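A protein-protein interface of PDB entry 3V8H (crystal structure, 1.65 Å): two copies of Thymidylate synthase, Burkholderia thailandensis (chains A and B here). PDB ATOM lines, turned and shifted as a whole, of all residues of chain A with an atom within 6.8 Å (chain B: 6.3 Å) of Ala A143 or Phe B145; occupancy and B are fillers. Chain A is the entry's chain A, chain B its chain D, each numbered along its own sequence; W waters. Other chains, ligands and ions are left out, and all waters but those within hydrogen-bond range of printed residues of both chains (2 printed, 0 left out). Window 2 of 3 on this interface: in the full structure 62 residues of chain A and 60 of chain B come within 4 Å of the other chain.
Ala A143 touches Phe B145, and with the chains exchanged Phe A145 touches Ala B143. Leu B154 touches its own counterpart, Leu A154. Of the 5 pairs that touch across the chains among the printed residues, 3 have their exchanged pair printed and touching as well.
Water W1 lies within hydrogen-bond range of the backbone carbonyl oxygen (O) of Arg B144 (2.7 Å) and the backbone carbonyl oxygen (O) of Arg A144 (2.9 Å). Water W2 bridges O of Glu B146 (2.7 Å) and O of Val A142 (2.9 Å).
Of the 11 printed residues of chain B, 4 touch a printed residue of chain A. Hydrophobic or aromatic side chains of chain B within 4 Å of the printed part of chain A: Ala B143, Phe B145 and Leu B154. Among the printed residues, 5 pairs touch across the chains.
Of chain B, only Phe B145 (3.4 Å) comes within 4 Å of Ala A143. Printed residues of chain A within 4 Å of Phe B145: Val A142 (3.8 Å) and Ala A143 (3.4 Å). Printed residues of chain A within 4 Å of Ala B143: Phe A145 (3.4 Å). Of the printed residues of chain A, Glu B147 touches Val A142 (3.6 Å). Printed residues of chain A within 4 Å of Leu B154: Leu A154. Asp B151 touches none of the printed residues of chain A. The nearest printed residue of chain B that does not touch Ala A143 is Glu B146 (6.0 Å).
N of Leu A154 lies within hydrogen-bond range of O of Ala A143 (2.9 Å). The backbone carbonyl oxygen of Leu A154 is in hydrogen-bond range of the backbone NH of Val A142 (2.8 Å). The backbone NH (N) of Lys B152 lies within hydrogen-bond range of the backbone carbonyl oxygen (O) of Phe B145 (2.7 Å). N of Leu B154 sits at hydrogen-bond distance from O of Ala B143 (2.9 Å). The backbone carbonyl oxygen of Phe A145 lies within hydrogen-bond range of the backbone NH of Lys A152 (2.7 Å).
Among the printed residues, merely in contact across the chains: Phe A145 with Ala B143 (3.4 Å), Ala A143 with Phe B145 (3.4 Å), Val A142 with Glu B147 (3.6 Å), Val A142 with Phe B145 (3.8 Å) and Leu A154 with Leu B154 (3.9 Å).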
ATOM      1  N   ARG A 140      -5.798 -32.991  18.883  1.00  0.00           N
ATOM      2  CA  ARG A 140      -5.352 -32.504  20.185  1.00  0.00           C
ATOM      3  C   ARG A 140      -5.483 -31.000  20.204  1.00  0.00           C
ATOM      4  O   ARG A 140      -5.350 -30.345  19.177  1.00  0.00           O
ATOM      5  CB  ARG A 140      -3.915 -32.990  20.455  1.00  0.00           C
ATOM      6  CG  ARG A 140      -3.774 -34.492  20.551  1.00  0.00           C
ATOM      7  CD  ARG A 140      -4.296 -35.064  21.875  1.00  0.00           C
ATOM      8  NE  ARG A 140      -4.142 -36.529  21.935  1.00  0.00           N
ATOM      9  CZ  ARG A 140      -5.007 -37.392  21.473  1.00  0.00           C
ATOM     10  NH1 ARG A 140      -6.110 -36.965  20.888  1.00  0.00           N
ATOM     11  NH2 ARG A 140      -4.789 -38.686  21.613  1.00  0.00           N
ATOM     12  N   ILE A 141      -5.790 -30.449  21.388  1.00  0.00           N
ATOM     13  CA  ILE A 141      -5.993 -29.017  21.586  1.00  0.00           C
ATOM     14  C   ILE A 141      -4.638 -28.327  21.630  1.00  0.00           C
ATOM     15  O   ILE A 141      -3.781 -28.647  22.462  1.00  0.00           O
ATOM     16  CB  ILE A 141      -6.750 -28.695  22.887  1.00  0.00           C
ATOM     17  CG1 ILE A 141      -8.126 -29.350  22.875  1.00  0.00           C
ATOM     18  CG2 ILE A 141      -6.835 -27.199  23.074  1.00  0.00           C
ATOM     19  CD1 ILE A 141      -8.810 -29.434  24.230  1.00  0.00           C
ATOM     20  N   VAL A 142      -4.439 -27.396  20.712  1.00  0.00           N
ATOM     21  CA  VAL A 142      -3.165 -26.713  20.601  1.00  0.00           C
ATOM     22  C   VAL A 142      -3.214 -25.248  20.999  1.00  0.00           C
ATOM     23  O   VAL A 142      -2.173 -24.617  21.177  1.00  0.00           O
ATOM     24  CB  VAL A 142      -2.594 -26.814  19.203  1.00  0.00           C
ATOM     25  CG1 VAL A 142      -2.302 -28.275  18.886  1.00  0.00           C
ATOM     26  CG2 VAL A 142      -3.519 -26.156  18.195  1.00  0.00           C
ATOM     27  N   ALA A 143      -4.414 -24.710  21.149  1.00  0.00           N
ATOM     28  CA  ALA A 143      -4.544 -23.309  21.558  1.00  0.00           C
ATOM     29  C   ALA A 143      -5.955 -23.018  22.029  1.00  0.00           C
ATOM     30  O   ALA A 143      -6.920 -23.656  21.614  1.00  0.00           O
ATOM     31  CB  ALA A 143      -4.180 -22.377  20.404  1.00  0.00           C
ATOM     32  N   ARG A 144      -6.052 -22.015  22.903  1.00  0.00           N
ATOM     33  CA  ARG A 144      -7.318 -21.475  23.373  1.00  0.00           C
ATOM     34  C   ARG A 144      -7.262 -19.984  23.091  1.00  0.00           C
ATOM     35  O   ARG A 144      -6.262 -19.337  23.413  1.00  0.00           O
ATOM     36  CB  ARG A 144      -7.464 -21.660  24.888  1.00  0.00           C
ATOM     37  CG  ARG A 144      -7.924 -23.034  25.292  1.00  0.00           C
ATOM     38  CD  ARG A 144      -7.251 -23.543  26.553  1.00  0.00           C
ATOM     39  NE  ARG A 144      -7.410 -25.001  26.632  1.00  0.00           N
ATOM     40  CZ  ARG A 144      -6.440 -25.905  26.481  1.00  0.00           C
ATOM     41  NH1 ARG A 144      -5.188 -25.529  26.251  1.00  0.00           N
ATOM     42  NH2 ARG A 144      -6.733 -27.212  26.579  1.00  0.00           N
ATOM     43  N   PHE A 145      -8.309 -19.435  22.501  1.00  0.00           N
ATOM     44  CA  PHE A 145      -8.304 -18.019  22.141  1.00  0.00           C
ATOM     45  C   PHE A 145      -9.720 -17.480  22.107  1.00  0.00           C
ATOM     46  O   PHE A 145     -10.680 -18.247  22.065  1.00  0.00           O
ATOM     47  CB  PHE A 145      -7.609 -17.792  20.792  1.00  0.00           C
ATOM     48  CG  PHE A 145      -8.269 -18.502  19.625  1.00  0.00           C
ATOM     49  CD1 PHE A 145      -8.023 -19.834  19.369  1.00  0.00           C
ATOM     50  CD2 PHE A 145      -9.115 -17.827  18.770  1.00  0.00           C
ATOM     51  CE1 PHE A 145      -8.615 -20.481  18.286  1.00  0.00           C
ATOM     52  CE2 PHE A 145      -9.712 -18.454  17.691  1.00  0.00           C
ATOM     53  CZ  PHE A 145      -9.470 -19.793  17.447  1.00  0.00           C
ATOM     54  N   LYS A 152     -12.772 -19.951  22.192  1.00  0.00           N
ATOM     55  CA  LYS A 152     -12.543 -21.023  21.205  1.00  0.00           C
ATOM     56  C   LYS A 152     -11.362 -21.915  21.571  1.00  0.00           C
ATOM     57  O   LYS A 152     -10.454 -21.504  22.289  1.00  0.00           O
ATOM     58  CB  LYS A 152     -12.228 -20.417  19.832  1.00  0.00           C
ATOM     59  CG  LYS A 152     -13.180 -19.339  19.351  1.00  0.00           C
ATOM     60  CD  LYS A 152     -14.559 -19.876  19.051  1.00  0.00           C
ATOM     61  CE  LYS A 152     -15.338 -18.915  18.156  1.00  0.00           C
ATOM     62  NZ  LYS A 152     -16.684 -19.455  17.795  1.00  0.00           N
ATOM     63  N   VAL A 153     -11.374 -23.138  21.030  1.00  0.00           N
ATOM     64  CA  VAL A 153     -10.207 -24.008  21.034  1.00  0.00           C
ATOM     65  C   VAL A 153      -9.819 -24.409  19.591  1.00  0.00           C
ATOM     66  O   VAL A 153     -10.675 -24.723  18.742  1.00  0.00           O
ATOM     67  CB  VAL A 153     -10.370 -25.245  21.934  1.00  0.00           C
ATOM     68  CG1 VAL A 153     -10.372 -24.814  23.405  1.00  0.00           C
ATOM     69  CG2 VAL A 153     -11.621 -26.048  21.568  1.00  0.00           C
ATOM     70  N   LEU A 154      -8.521 -24.362  19.309  1.00  0.00           N
ATOM     71  CA  LEU A 154      -7.961 -24.917  18.074  1.00  0.00           C
ATOM     72  C   LEU A 154      -7.499 -26.342  18.320  1.00  0.00           C
ATOM     73  O   LEU A 154      -6.712 -26.619  19.253  1.00  0.00           O
ATOM     74  CB  LEU A 154      -6.753 -24.114  17.619  1.00  0.00           C
ATOM     75  CG  LEU A 154      -6.075 -24.588  16.341  1.00  0.00           C
ATOM     76  CD1 LEU A 154      -6.944 -24.460  15.084  1.00  0.00           C
ATOM     77  CD2 LEU A 154      -4.766 -23.840  16.139  1.00  0.00           C
ATOM     78  N   LEU A 155      -8.026 -27.259  17.523  1.00  0.00           N
ATOM     79  CA  LEU A 155      -7.570 -28.636  17.533  1.00  0.00           C
ATOM     80  C   LEU A 155      -6.810 -28.964  16.254  1.00  0.00           C
ATOM     81  O   LEU A 155      -7.138 -28.441  15.186  1.00  0.00           O
ATOM     82  CB  LEU A 155      -8.737 -29.592  17.670  1.00  0.00           C
ATOM     83  CG  LEU A 155      -9.331 -29.592  19.092  1.00  0.00           C
ATOM     84  CD1 LEU A 155     -10.338 -28.464  19.383  1.00  0.00           C
ATOM     85  CD2 LEU A 155      -9.936 -30.957  19.307  1.00  0.00           C
ATOM     86  N   VAL B 122      -0.902 -22.447  10.471  1.00  0.00           N
ATOM     87  CA  VAL B 122      -0.260 -22.034  11.700  1.00  0.00           C
ATOM     88  C   VAL B 122       1.162 -21.641  11.319  1.00  0.00           C
ATOM     89  O   VAL B 122       1.932 -22.496  10.856  1.00  0.00           O
ATOM     90  CB  VAL B 122      -0.277 -23.140  12.768  1.00  0.00           C
ATOM     91  CG1 VAL B 122       0.521 -22.732  13.998  1.00  0.00           C
ATOM     92  CG2 VAL B 122      -1.721 -23.425  13.197  1.00  0.00           C
ATOM     93  N   ALA B 143      -6.003 -15.768  15.456  1.00  0.00           N
ATOM     94  CA  ALA B 143      -5.567 -16.066  16.820  1.00  0.00           C
ATOM     95  C   ALA B 143      -4.058 -16.008  16.929  1.00  0.00           C
ATOM     96  O   ALA B 143      -3.343 -16.194  15.941  1.00  0.00           O
ATOM     97  CB  ALA B 143      -6.091 -17.431  17.269  1.00  0.00           C
ATOM     98  N   ARG B 144      -3.591 -15.694  18.145  1.00  0.00           N
ATOM     99  CA  ARG B 144      -2.162 -15.740  18.516  1.00  0.00           C
ATOM    100  C   ARG B 144      -2.024 -16.574  19.789  1.00  0.00           C
ATOM    101  O   ARG B 144      -2.872 -16.489  20.695  1.00  0.00           O
ATOM    102  CB  ARG B 144      -1.634 -14.369  18.830  1.00  0.00           C
ATOM    103  CG  ARG B 144      -1.545 -13.459  17.666  1.00  0.00           C
ATOM    104  CD  ARG B 144      -1.086 -12.051  18.086  1.00  0.00           C
ATOM    105  NE  ARG B 144      -1.032 -11.361  16.839  1.00  0.00           N
ATOM    106  CZ  ARG B 144      -0.005 -11.332  16.005  1.00  0.00           C
ATOM    107  NH1 ARG B 144       1.187 -11.819  16.322  1.00  0.00           N
ATOM    108  NH2 ARG B 144      -0.165 -10.737  14.848  1.00  0.00           N
ATOM    109  N   PHE B 145      -0.968 -17.373  19.842  1.00  0.00           N
ATOM    110  CA  PHE B 145      -0.785 -18.353  20.895  1.00  0.00           C
ATOM    111  C   PHE B 145       0.650 -18.832  20.897  1.00  0.00           C
ATOM    112  O   PHE B 145       1.364 -18.656  19.929  1.00  0.00           O
ATOM    113  CB  PHE B 145      -1.753 -19.531  20.725  1.00  0.00           C
ATOM    114  CG  PHE B 145      -1.558 -20.350  19.472  1.00  0.00           C
ATOM    115  CD1 PHE B 145      -2.167 -20.001  18.265  1.00  0.00           C
ATOM    116  CD2 PHE B 145      -0.812 -21.506  19.512  1.00  0.00           C
ATOM    117  CE1 PHE B 145      -2.022 -20.800  17.149  1.00  0.00           C
ATOM    118  CE2 PHE B 145      -0.656 -22.311  18.402  1.00  0.00           C
ATOM    119  CZ  PHE B 145      -1.240 -21.944  17.203  1.00  0.00           C
ATOM    120  N   GLU B 146       1.049 -19.460  22.007  1.00  0.00           N
ATOM    121  CA  GLU B 146       2.380 -20.007  22.177  1.00  0.00           C
ATOM    122  C   GLU B 146       2.260 -21.534  22.131  1.00  0.00           C
ATOM    123  O   GLU B 146       1.348 -22.112  22.750  1.00  0.00           O
ATOM    124  CB  GLU B 146       2.974 -19.540  23.521  1.00  0.00           C
ATOM    125  CG  GLU B 146       4.438 -19.907  23.689  1.00  0.00           C
ATOM    126  CD  GLU B 146       5.075 -19.401  24.988  1.00  0.00           C
ATOM    127  OE1 GLU B 146       4.374 -18.826  25.858  1.00  0.00           O
ATOM    128  OE2 GLU B 146       6.306 -19.586  25.129  1.00  0.00           O
ATOM    129  N   GLU B 147       3.113 -22.163  21.342  1.00  0.00           N
ATOM    130  CA  GLU B 147       3.178 -23.607  21.246  1.00  0.00           C
ATOM    131  C   GLU B 147       4.648 -23.992  21.125  1.00  0.00           C
ATOM    132  O   GLU B 147       5.377 -23.418  20.307  1.00  0.00           O
ATOM    133  CB  GLU B 147       2.395 -24.088  20.025  1.00  0.00           C
ATOM    134  CG  GLU B 147       2.565 -25.577  19.725  1.00  0.00           C
ATOM    135  CD  GLU B 147       1.753 -26.034  18.539  1.00  0.00           C
ATOM    136  OE1 GLU B 147       1.775 -25.345  17.504  1.00  0.00           O
ATOM    137  OE2 GLU B 147       1.109 -27.112  18.654  1.00  0.00           O
ATOM    138  N   ALA B 150       7.293 -21.288  21.016  1.00  0.00           N
ATOM    139  CA  ALA B 150       7.310 -20.339  19.885  1.00  0.00           C
ATOM    140  C   ALA B 150       5.997 -19.576  19.837  1.00  0.00           C
ATOM    141  O   ALA B 150       4.937 -20.121  20.126  1.00  0.00           O
ATOM    142  CB  ALA B 150       7.542 -21.066  18.573  1.00  0.00           C
ATOM    143  N   ASP B 151       6.070 -18.309  19.453  1.00  0.00           N
ATOM    144  CA  ASP B 151       4.869 -17.496  19.274  1.00  0.00           C
ATOM    145  C   ASP B 151       4.329 -17.812  17.910  1.00  0.00           C
ATOM    146  O   ASP B 151       5.070 -17.693  16.942  1.00  0.00           O
ATOM    147  CB  ASP B 151       5.234 -16.025  19.302  1.00  0.00           C
ATOM    148  CG  ASP B 151       5.850 -15.627  20.610  1.00  0.00           C
ATOM    149  OD1 ASP B 151       5.174 -15.821  21.638  1.00  0.00           O
ATOM    150  OD2 ASP B 151       7.006 -15.156  20.589  1.00  0.00           O
ATOM    151  N   LYS B 152       3.046 -18.200  17.839  1.00  0.00           N
ATOM    152  CA  LYS B 152       2.455 -18.554  16.568  1.00  0.00           C
ATOM    153  C   LYS B 152       1.210 -17.721  16.287  1.00  0.00           C
ATOM    154  O   LYS B 152       0.638 -17.085  17.180  1.00  0.00           O
ATOM    155  CB  LYS B 152       2.152 -20.057  16.509  1.00  0.00           C
ATOM    156  CG  LYS B 152       3.380 -20.954  16.720  1.00  0.00           C
ATOM    157  CD  LYS B 152       4.150 -21.257  15.445  1.00  0.00           C
ATOM    158  CE  LYS B 152       4.790 -22.654  15.468  1.00  0.00           C
ATOM    159  NZ  LYS B 152       5.561 -22.949  14.211  1.00  0.00           N
ATOM    160  N   VAL B 153       0.850 -17.681  15.016  1.00  0.00           N
ATOM    161  CA  VAL B 153      -0.396 -17.069  14.575  1.00  0.00           C
ATOM    162  C   VAL B 153      -1.192 -18.124  13.809  1.00  0.00           C
ATOM    163  O   VAL B 153      -0.621 -18.876  13.038  1.00  0.00           O
ATOM    164  CB  VAL B 153      -0.182 -15.858  13.664  1.00  0.00           C
ATOM    165  CG1 VAL B 153       0.289 -14.666  14.475  1.00  0.00           C
ATOM    166  CG2 VAL B 153       0.788 -16.163  12.536  1.00  0.00           C
ATOM    167  N   LEU B 154      -2.510 -18.134  14.006  1.00  0.00           N
ATOM    168  CA  LEU B 154      -3.432 -18.965  13.232  1.00  0.00           C
ATOM    169  C   LEU B 154      -4.056 -18.048  12.175  1.00  0.00           C
ATOM    170  O   LEU B 154      -4.566 -16.976  12.540  1.00  0.00           O
ATOM    171  CB  LEU B 154      -4.549 -19.470  14.141  1.00  0.00           C
ATOM    172  CG  LEU B 154      -5.633 -20.292  13.440  1.00  0.00           C
ATOM    173  CD1 LEU B 154      -5.096 -21.576  12.853  1.00  0.00           C
ATOM    174  CD2 LEU B 154      -6.764 -20.575  14.444  1.00  0.00           C
HETATM  175  O   HOH W   1      -4.038 -17.621  22.865  1.00  0.00           O
HETATM  176  O   HOH W   2      -0.927 -23.386  23.531  1.00  0.00           O
